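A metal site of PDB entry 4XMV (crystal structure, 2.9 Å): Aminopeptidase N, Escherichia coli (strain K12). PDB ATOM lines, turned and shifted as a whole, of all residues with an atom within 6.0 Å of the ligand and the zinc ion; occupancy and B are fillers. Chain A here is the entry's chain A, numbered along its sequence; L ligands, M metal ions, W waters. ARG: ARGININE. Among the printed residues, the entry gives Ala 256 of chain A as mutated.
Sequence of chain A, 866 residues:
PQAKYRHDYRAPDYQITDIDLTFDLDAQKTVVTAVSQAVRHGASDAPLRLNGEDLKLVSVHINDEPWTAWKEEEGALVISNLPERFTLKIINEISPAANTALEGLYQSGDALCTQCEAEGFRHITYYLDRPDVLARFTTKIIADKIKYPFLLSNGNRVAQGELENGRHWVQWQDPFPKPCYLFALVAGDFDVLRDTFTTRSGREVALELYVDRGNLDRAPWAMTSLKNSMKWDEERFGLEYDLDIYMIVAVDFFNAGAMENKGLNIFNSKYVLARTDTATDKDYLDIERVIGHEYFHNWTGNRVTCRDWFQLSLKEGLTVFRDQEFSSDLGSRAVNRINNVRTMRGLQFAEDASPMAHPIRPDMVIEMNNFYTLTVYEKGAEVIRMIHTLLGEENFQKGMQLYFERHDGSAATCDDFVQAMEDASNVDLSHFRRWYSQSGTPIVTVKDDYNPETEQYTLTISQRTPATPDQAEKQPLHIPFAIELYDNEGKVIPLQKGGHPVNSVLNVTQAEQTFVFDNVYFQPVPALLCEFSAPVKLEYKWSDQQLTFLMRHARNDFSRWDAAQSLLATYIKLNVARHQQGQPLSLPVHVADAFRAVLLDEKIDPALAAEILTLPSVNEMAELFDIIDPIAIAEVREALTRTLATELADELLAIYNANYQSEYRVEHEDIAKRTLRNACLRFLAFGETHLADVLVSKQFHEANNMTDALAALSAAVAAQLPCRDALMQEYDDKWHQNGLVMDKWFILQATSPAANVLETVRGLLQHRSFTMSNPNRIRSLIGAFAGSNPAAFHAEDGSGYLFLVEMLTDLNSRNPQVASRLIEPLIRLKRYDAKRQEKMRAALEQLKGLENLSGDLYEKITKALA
O of Ala 258 sits close to O of the ligand, 3.4 Å away. Gln 115 touches the ligand (CG to NH1, 3.8 Å). Ala 256 touches the ligand. Met 259 touches the ligand (SD to N, 3.9 Å). Lys 315 touches the ligand (NZ to N, 3.7 Å). Asn 369 touches the ligand. Tyr 372 touches the ligand. Hydrophobic or aromatic side chains within 4 Å of the ligand: Ala 256, Met 259, His 293, Tyr 372 and Tyr 377. Within 4 Å of the ligand: Gln 115, Glu 117, Ala 256, Ala 258, Met 259, Glu 260, His 293, Glu 294, His 297, Lys 315, Glu 316, Asn 369, Tyr 372, Tyr 377 and Gln 817. The nearest printed residue that does not touch the ligand is Ala 118 (4.7 Å).
Within 4 Å of the zinc ion: His 293, His 297 and Glu 316. The nearest printed residue that does not touch the zinc ion is Tyr 377 (4.04 Å).
The side-chain hydroxyl (OH) of Tyr 377 lies within hydrogen-bond range of the side-chain carboxylate (OE2) of Glu 316, 3.2 Å away. The side-chain carboxylate of Glu 316 lies within salt-bridge range of the side-chain amino group of Lys 315, at 3.1 Å. OE1 of Glu 260 is in salt-bridge range of NZ of Lys 315, 3.4 Å away. The side-chain carboxylate (OE2) of Glu 117 sits at hydrogen-bond distance from the side-chain hydroxyl (OH) of Tyr 372 (2.6 Å). The backbone carbonyl oxygen (O) of Glu 117 is in hydrogen-bond range of the side-chain amide nitrogen (NE2) of Gln 115, at 3.2 Å. The side-chain amide oxygen (OD1) of Asn 369 sits at hydrogen-bond distance from the side-chain amide nitrogen (NE2) of Gln 817 (2.9 Å). The side-chain hydroxyl of Thr 319 is in hydrogen-bond range of the backbone carbonyl oxygen of Lys 315 (2.5 Å). The side-chain sulfur of Met 259 sits at hydrogen-bond distance from the side-chain amide nitrogen of Gln 115 (3.3 Å).
OE2 of Glu 294 lies close to O of the ligand. The side-chain carboxylate (OE1) of Glu 260 is in salt-bridge range of a nitrogen (N) of the ligand (2.5 Å). A nitrogen (NH1) of the ligand is in hydrogen-bond range of the backbone carbonyl oxygen (O) of Glu 117 (3.3 Å). The side-chain carboxylate (OE1) of Glu 117 lies within salt-bridge range of a nitrogen (N) of the ligand, at 2.7 Å. OXT of the ligand sits close to OH of Tyr 377 (2.8 Å). A nitrogen (NH1) of the ligand lies within hydrogen-bond range of the side-chain amide oxygen of Gln 817 (3.4 Å).
The zinc ion is bound by an oxygen (OXT) of the ligand (1.8 Å). OE1 of Glu 316 is bound to the zinc ion. NE2 of His 293 is bound to the zinc ion (2.1 Å). The zinc ion is bound by a ring nitrogen (NE2) of His 297 (2.1 Å). The zinc ion has four donor atoms within binding distance. Slightly farther from the zinc ion lies the side-chain carboxylate (OE2) of Glu 316 (2.8 Å).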
ATOM      1  N   LEU A 102      33.670  10.474 -23.071  1.00  0.00           N
ATOM      2  CA  LEU A 102      32.607  11.440 -23.321  1.00  0.00           C
ATOM      3  C   LEU A 102      31.465  11.321 -22.313  1.00  0.00           C
ATOM      4  O   LEU A 102      30.300  11.487 -22.692  1.00  0.00           O
ATOM      5  CB  LEU A 102      32.116  11.407 -24.791  1.00  0.00           C
ATOM      6  CG  LEU A 102      33.177  11.365 -25.918  1.00  0.00           C
ATOM      7  CD1 LEU A 102      32.512  11.371 -27.291  1.00  0.00           C
ATOM      8  CD2 LEU A 102      34.204  12.490 -25.849  1.00  0.00           C
ATOM      9  N   GLN A 115      27.998  15.618 -20.692  1.00  0.00           N
ATOM     10  CA  GLN A 115      26.941  14.608 -20.638  1.00  0.00           C
ATOM     11  C   GLN A 115      26.903  13.969 -19.232  1.00  0.00           C
ATOM     12  O   GLN A 115      27.891  13.383 -18.771  1.00  0.00           O
ATOM     13  CB  GLN A 115      27.104  13.566 -21.734  1.00  0.00           C
ATOM     14  CG  GLN A 115      26.007  12.540 -21.771  1.00  0.00           C
ATOM     15  CD  GLN A 115      24.617  13.139 -21.876  1.00  0.00           C
ATOM     16  OE1 GLN A 115      24.416  14.161 -22.548  1.00  0.00           O
ATOM     17  NE2 GLN A 115      23.649  12.495 -21.233  1.00  0.00           N
ATOM     18  N   GLU A 117      23.746  12.355 -17.875  1.00  0.00           N
ATOM     19  CA  GLU A 117      22.887  11.171 -17.809  1.00  0.00           C
ATOM     20  C   GLU A 117      23.745   9.987 -18.273  1.00  0.00           C
ATOM     21  O   GLU A 117      24.456  10.093 -19.264  1.00  0.00           O
ATOM     22  CB  GLU A 117      21.579  11.322 -18.631  1.00  0.00           C
ATOM     23  CG  GLU A 117      20.603  10.174 -18.380  1.00  0.00           C
ATOM     24  CD  GLU A 117      19.255  10.278 -19.068  1.00  0.00           C
ATOM     25  OE1 GLU A 117      19.070  11.164 -19.915  1.00  0.00           O
ATOM     26  OE2 GLU A 117      18.360   9.441 -18.782  1.00  0.00           O
ATOM     27  N   ALA A 118      23.701   8.872 -17.532  1.00  0.00           N
ATOM     28  CA  ALA A 118      22.890   8.715 -16.302  1.00  0.00           C
ATOM     29  C   ALA A 118      23.673   9.122 -15.070  1.00  0.00           C
ATOM     30  O   ALA A 118      23.154   9.855 -14.204  1.00  0.00           O
ATOM     31  CB  ALA A 118      22.379   7.275 -16.152  1.00  0.00           C
ATOM     32  N   PHE A 254      29.626  13.108 -29.634  1.00  0.00           N
ATOM     33  CA  PHE A 254      28.548  12.699 -28.731  1.00  0.00           C
ATOM     34  C   PHE A 254      28.255  11.224 -28.881  1.00  0.00           C
ATOM     35  O   PHE A 254      28.208  10.697 -29.986  1.00  0.00           O
ATOM     36  CB  PHE A 254      27.313  13.483 -29.089  1.00  0.00           C
ATOM     37  CG  PHE A 254      26.371  13.670 -27.963  1.00  0.00           C
ATOM     38  CD1 PHE A 254      26.644  14.597 -26.974  1.00  0.00           C
ATOM     39  CD2 PHE A 254      25.185  12.952 -27.914  1.00  0.00           C
ATOM     40  CE1 PHE A 254      25.771  14.787 -25.931  1.00  0.00           C
ATOM     41  CE2 PHE A 254      24.297  13.141 -26.880  1.00  0.00           C
ATOM     42  CZ  PHE A 254      24.597  14.076 -25.882  1.00  0.00           C
ATOM     43  N   ASN A 255      28.061  10.533 -27.784  1.00  0.00           N
ATOM     44  CA  ASN A 255      27.838   9.125 -27.860  1.00  0.00           C
ATOM     45  C   ASN A 255      26.465   8.734 -28.391  1.00  0.00           C
ATOM     46  O   ASN A 255      26.355   7.827 -29.261  1.00  0.00           O
ATOM     47  CB  ASN A 255      28.096   8.504 -26.505  1.00  0.00           C
ATOM     48  CG  ASN A 255      29.558   8.503 -26.172  1.00  0.00           C
ATOM     49  OD1 ASN A 255      30.390   8.536 -27.057  1.00  0.00           O
ATOM     50  ND2 ASN A 255      29.889   8.460 -24.886  1.00  0.00           N
ATOM     51  N   ALA A 256      25.422   9.397 -27.905  1.00  0.00           N
ATOM     52  CA  ALA A 256      24.068   9.082 -28.356  1.00  0.00           C
ATOM     53  C   ALA A 256      23.471  10.181 -29.249  1.00  0.00           C
ATOM     54  O   ALA A 256      24.159  10.669 -30.154  1.00  0.00           O
ATOM     55  CB  ALA A 256      23.159   8.785 -27.162  1.00  0.00           C
ATOM     56  N   GLY A 257      22.215  10.563 -28.991  1.00  0.00           N
ATOM     57  CA  GLY A 257      21.444  11.350 -29.930  1.00  0.00           C
ATOM     58  C   GLY A 257      21.353  12.780 -29.504  1.00  0.00           C
ATOM     59  O   GLY A 257      21.796  13.678 -30.200  1.00  0.00           O
ATOM     60  N   ALA A 258      20.736  12.975 -28.349  1.00  0.00           N
ATOM     61  CA  ALA A 258      20.611  14.281 -27.748  1.00  0.00           C
ATOM     62  C   ALA A 258      20.325  14.107 -26.241  1.00  0.00           C
ATOM     63  O   ALA A 258      20.244  12.986 -25.735  1.00  0.00           O
ATOM     64  CB  ALA A 258      19.528  15.084 -28.443  1.00  0.00           C
ATOM     65  N   MET A 259      20.249  15.225 -25.518  1.00  0.00           N
ATOM     66  CA  MET A 259      20.042  15.214 -24.097  1.00  0.00           C
ATOM     67  C   MET A 259      19.169  16.397 -23.674  1.00  0.00           C
ATOM     68  O   MET A 259      19.402  17.530 -24.085  1.00  0.00           O
ATOM     69  CB  MET A 259      21.394  15.220 -23.423  1.00  0.00           C
ATOM     70  CG  MET A 259      21.336  15.124 -21.898  1.00  0.00           C
ATOM     71  SD  MET A 259      20.595  13.612 -21.258  1.00  0.00           S
ATOM     72  CE  MET A 259      19.638  14.218 -19.881  1.00  0.00           C
ATOM     73  N   GLU A 260      18.210  16.119 -22.792  1.00  0.00           N
ATOM     74  CA  GLU A 260      17.155  17.057 -22.370  1.00  0.00           C
ATOM     75  C   GLU A 260      17.543  17.974 -21.218  1.00  0.00           C
ATOM     76  O   GLU A 260      16.679  18.392 -20.464  1.00  0.00           O
ATOM     77  CB  GLU A 260      15.900  16.310 -21.848  1.00  0.00           C
ATOM     78  CG  GLU A 260      15.859  14.795 -22.091  1.00  0.00           C
ATOM     79  CD  GLU A 260      16.099  13.911 -20.876  1.00  0.00           C
ATOM     80  OE1 GLU A 260      16.936  13.023 -21.094  1.00  0.00           O
ATOM     81  OE2 GLU A 260      15.471  14.063 -19.775  1.00  0.00           O
ATOM     82  N   VAL A 290      13.659  13.983 -32.995  1.00  0.00           N
ATOM     83  CA  VAL A 290      14.527  14.125 -31.836  1.00  0.00           C
ATOM     84  C   VAL A 290      14.427  15.495 -31.163  1.00  0.00           C
ATOM     85  O   VAL A 290      14.406  15.569 -29.927  1.00  0.00           O
ATOM     86  CB  VAL A 290      15.989  13.801 -32.206  1.00  0.00           C
ATOM     87  CG1 VAL A 290      16.960  14.092 -31.066  1.00  0.00           C
ATOM     88  CG2 VAL A 290      16.093  12.327 -32.623  1.00  0.00           C
ATOM     89  N   HIS A 293      11.442  15.118 -29.277  1.00  0.00           N
ATOM     90  CA  HIS A 293      11.672  14.171 -28.184  1.00  0.00           C
ATOM     91  C   HIS A 293      12.255  14.905 -27.024  1.00  0.00           C
ATOM     92  O   HIS A 293      11.703  14.826 -25.955  1.00  0.00           O
ATOM     93  CB  HIS A 293      12.609  13.035 -28.620  1.00  0.00           C
ATOM     94  CG  HIS A 293      12.828  11.977 -27.558  1.00  0.00           C
ATOM     95  ND1 HIS A 293      12.016  10.862 -27.423  1.00  0.00           N
ATOM     96  CD2 HIS A 293      13.766  11.869 -26.578  1.00  0.00           C
ATOM     97  CE1 HIS A 293      12.434  10.129 -26.404  1.00  0.00           C
ATOM     98  NE2 HIS A 293      13.487  10.722 -25.877  1.00  0.00           N
ATOM     99  N   GLU A 294      13.355  15.654 -27.231  1.00  0.00           N
ATOM    100  CA  GLU A 294      14.021  16.311 -26.118  1.00  0.00           C
ATOM    101  C   GLU A 294      13.191  17.455 -25.555  1.00  0.00           C
ATOM    102  O   GLU A 294      13.267  17.819 -24.368  1.00  0.00           O
ATOM    103  CB  GLU A 294      15.408  16.846 -26.516  1.00  0.00           C
ATOM    104  CG  GLU A 294      16.431  15.841 -27.056  1.00  0.00           C
ATOM    105  CD  GLU A 294      16.490  14.540 -26.285  1.00  0.00           C
ATOM    106  OE1 GLU A 294      16.035  14.506 -25.114  1.00  0.00           O
ATOM    107  OE2 GLU A 294      16.974  13.536 -26.843  1.00  0.00           O
ATOM    108  N   HIS A 297      10.531  15.986 -23.223  1.00  0.00           N
ATOM    109  CA  HIS A 297      11.133  15.614 -21.940  1.00  0.00           C
ATOM    110  C   HIS A 297      11.002  16.688 -20.870  1.00  0.00           C
ATOM    111  O   HIS A 297      11.130  16.410 -19.677  1.00  0.00           O
ATOM    112  CB  HIS A 297      12.617  15.246 -22.108  1.00  0.00           C
ATOM    113  CG  HIS A 297      12.866  13.780 -22.270  1.00  0.00           C
ATOM    114  ND1 HIS A 297      12.524  12.871 -21.306  1.00  0.00           N
ATOM    115  CD2 HIS A 297      13.442  13.076 -23.271  1.00  0.00           C
ATOM    116  CE1 HIS A 297      12.864  11.657 -21.706  1.00  0.00           C
ATOM    117  NE2 HIS A 297      13.430  11.755 -22.895  1.00  0.00           N
ATOM    118  N   LYS A 315      10.083   7.913 -18.090  1.00  0.00           N
ATOM    119  CA  LYS A 315      10.310   9.053 -18.978  1.00  0.00           C
ATOM    120  C   LYS A 315      10.573   8.709 -20.478  1.00  0.00           C
ATOM    121  O   LYS A 315      10.044   9.379 -21.364  1.00  0.00           O
ATOM    122  CB  LYS A 315      11.412   9.973 -18.423  1.00  0.00           C
ATOM    123  CG  LYS A 315      12.841   9.440 -18.409  1.00  0.00           C
ATOM    124  CD  LYS A 315      13.797  10.504 -17.848  1.00  0.00           C
ATOM    125  CE  LYS A 315      15.277  10.095 -17.909  1.00  0.00           C
ATOM    126  NZ  LYS A 315      15.905  10.392 -19.230  1.00  0.00           N
ATOM    127  N   GLU A 316      11.367   7.696 -20.772  1.00  0.00           N
ATOM    128  CA  GLU A 316      11.648   7.350 -22.140  1.00  0.00           C
ATOM    129  C   GLU A 316      10.487   6.655 -22.842  1.00  0.00           C
ATOM    130  O   GLU A 316      10.226   6.866 -24.014  1.00  0.00           O
ATOM    131  CB  GLU A 316      12.883   6.465 -22.223  1.00  0.00           C
ATOM    132  CG  GLU A 316      14.158   7.115 -21.708  1.00  0.00           C
ATOM    133  CD  GLU A 316      14.482   8.448 -22.373  1.00  0.00           C
ATOM    134  OE1 GLU A 316      13.788   8.887 -23.313  1.00  0.00           O
ATOM    135  OE2 GLU A 316      15.471   9.076 -21.950  1.00  0.00           O
ATOM    136  N   THR A 319       8.010   9.520 -23.335  1.00  0.00           N
ATOM    137  CA  THR A 319       8.499  10.616 -24.171  1.00  0.00           C
ATOM    138  C   THR A 319       8.594  10.167 -25.626  1.00  0.00           C
ATOM    139  O   THR A 319       8.249  10.927 -26.534  1.00  0.00           O
ATOM    140  CB  THR A 319       9.844  11.185 -23.646  1.00  0.00           C
ATOM    141  OG1 THR A 319       9.698  11.625 -22.286  1.00  0.00           O
ATOM    142  CG2 THR A 319      10.285  12.368 -24.472  1.00  0.00           C
ATOM    143  N   VAL A 320       9.017   8.911 -25.838  1.00  0.00           N
ATOM    144  CA  VAL A 320       8.997   8.293 -27.180  1.00  0.00           C
ATOM    145  C   VAL A 320       7.567   8.238 -27.733  1.00  0.00           C
ATOM    146  O   VAL A 320       7.290   8.652 -28.867  1.00  0.00           O
ATOM    147  CB  VAL A 320       9.581   6.863 -27.163  1.00  0.00           C
ATOM    148  CG1 VAL A 320       9.251   6.088 -28.440  1.00  0.00           C
ATOM    149  CG2 VAL A 320      11.090   6.911 -27.000  1.00  0.00           C
ATOM    150  N   ASN A 369      24.220   2.605 -18.681  1.00  0.00           N
ATOM    151  CA  ASN A 369      24.051   2.986 -20.087  1.00  0.00           C
ATOM    152  C   ASN A 369      23.607   1.809 -20.875  1.00  0.00           C
ATOM    153  O   ASN A 369      23.039   1.978 -21.948  1.00  0.00           O
ATOM    154  CB  ASN A 369      25.283   3.549 -20.731  1.00  0.00           C
ATOM    155  CG  ASN A 369      25.567   4.930 -20.249  1.00  0.00           C
ATOM    156  OD1 ASN A 369      26.633   5.144 -19.664  1.00  0.00           O
ATOM    157  ND2 ASN A 369      24.613   5.865 -20.426  1.00  0.00           N
ATOM    158  N   TYR A 372      19.754   1.804 -22.043  1.00  0.00           N
ATOM    159  CA  TYR A 372      19.198   2.814 -22.933  1.00  0.00           C
ATOM    160  C   TYR A 372      18.852   2.124 -24.232  1.00  0.00           C
ATOM    161  O   TYR A 372      19.422   2.381 -25.272  1.00  0.00           O
ATOM    162  CB  TYR A 372      20.173   3.999 -23.073  1.00  0.00           C
ATOM    163  CG  TYR A 372      20.091   4.903 -21.837  1.00  0.00           C
ATOM    164  CD1 TYR A 372      20.800   4.584 -20.691  1.00  0.00           C
ATOM    165  CD2 TYR A 372      19.240   6.001 -21.808  1.00  0.00           C
ATOM    166  CE1 TYR A 372      20.682   5.346 -19.553  1.00  0.00           C
ATOM    167  CE2 TYR A 372      19.109   6.776 -20.660  1.00  0.00           C
ATOM    168  CZ  TYR A 372      19.846   6.447 -19.548  1.00  0.00           C
ATOM    169  OH  TYR A 372      19.726   7.213 -18.420  1.00  0.00           O
ATOM    170  N   TYR A 377      12.982   2.065 -24.434  1.00  0.00           N
ATOM    171  CA  TYR A 377      12.481   3.143 -25.291  1.00  0.00           C
ATOM    172  C   TYR A 377      11.235   2.712 -26.068  1.00  0.00           C
ATOM    173  O   TYR A 377      10.144   3.175 -25.787  1.00  0.00           O
ATOM    174  CB  TYR A 377      13.557   3.638 -26.264  1.00  0.00           C
ATOM    175  CG  TYR A 377      14.523   4.665 -25.679  1.00  0.00           C
ATOM    176  CD1 TYR A 377      15.403   4.313 -24.695  1.00  0.00           C
ATOM    177  CD2 TYR A 377      14.560   5.981 -26.156  1.00  0.00           C
ATOM    178  CE1 TYR A 377      16.319   5.230 -24.187  1.00  0.00           C
ATOM    179  CE2 TYR A 377      15.459   6.916 -25.647  1.00  0.00           C
ATOM    180  CZ  TYR A 377      16.327   6.540 -24.649  1.00  0.00           C
ATOM    181  OH  TYR A 377      17.225   7.445 -24.120  1.00  0.00           O
ATOM    182  N   GLN A 817      31.004   3.078 -23.699  1.00  0.00           N
ATOM    183  CA  GLN A 817      29.608   3.169 -24.129  1.00  0.00           C
ATOM    184  C   GLN A 817      29.428   2.839 -25.607  1.00  0.00           C
ATOM    185  O   GLN A 817      28.486   2.129 -25.991  1.00  0.00           O
ATOM    186  CB  GLN A 817      29.074   4.561 -23.902  1.00  0.00           C
ATOM    187  CG  GLN A 817      29.052   5.004 -22.455  1.00  0.00           C
ATOM    188  CD  GLN A 817      28.223   6.260 -22.260  1.00  0.00           C
ATOM    189  OE1 GLN A 817      27.433   6.637 -23.115  1.00  0.00           O
ATOM    190  NE2 GLN A 817      28.392   6.893 -21.119  1.00  0.00           N
HETATM  191  N   ARG L   1      17.885  11.020 -22.317  1.00  0.00           N
HETATM  192  CA  ARG L   1      18.439  10.975 -23.690  1.00  0.00           C
HETATM  193  C   ARG L   1      17.290  10.784 -24.679  1.00  0.00           C
HETATM  194  O   ARG L   1      17.279  11.278 -25.814  1.00  0.00           O
HETATM  195  CB  ARG L   1      19.477   9.842 -23.840  1.00  0.00           C
HETATM  196  CG  ARG L   1      20.729   9.977 -22.974  1.00  0.00           C
HETATM  197  CD  ARG L   1      21.345   8.615 -22.667  1.00  0.00           C
HETATM  198  NE  ARG L   1      22.705   8.636 -22.126  1.00  0.00           N
HETATM  199  CZ  ARG L   1      23.787   8.920 -22.840  1.00  0.00           C
HETATM  200  NH1 ARG L   1      24.988   8.895 -22.272  1.00  0.00           N
HETATM  201  NH2 ARG L   1      23.687   9.254 -24.115  1.00  0.00           N
HETATM  202  OXT ARG L   1      16.325  10.113 -24.350  1.00  0.00           O
HETATM  203 ZN    ZN M   1      14.584  10.564 -24.135  1.00  0.00          ZN
HETATM  204  O   HOH W   1      17.661   9.840 -28.231  1.00  0.00           O
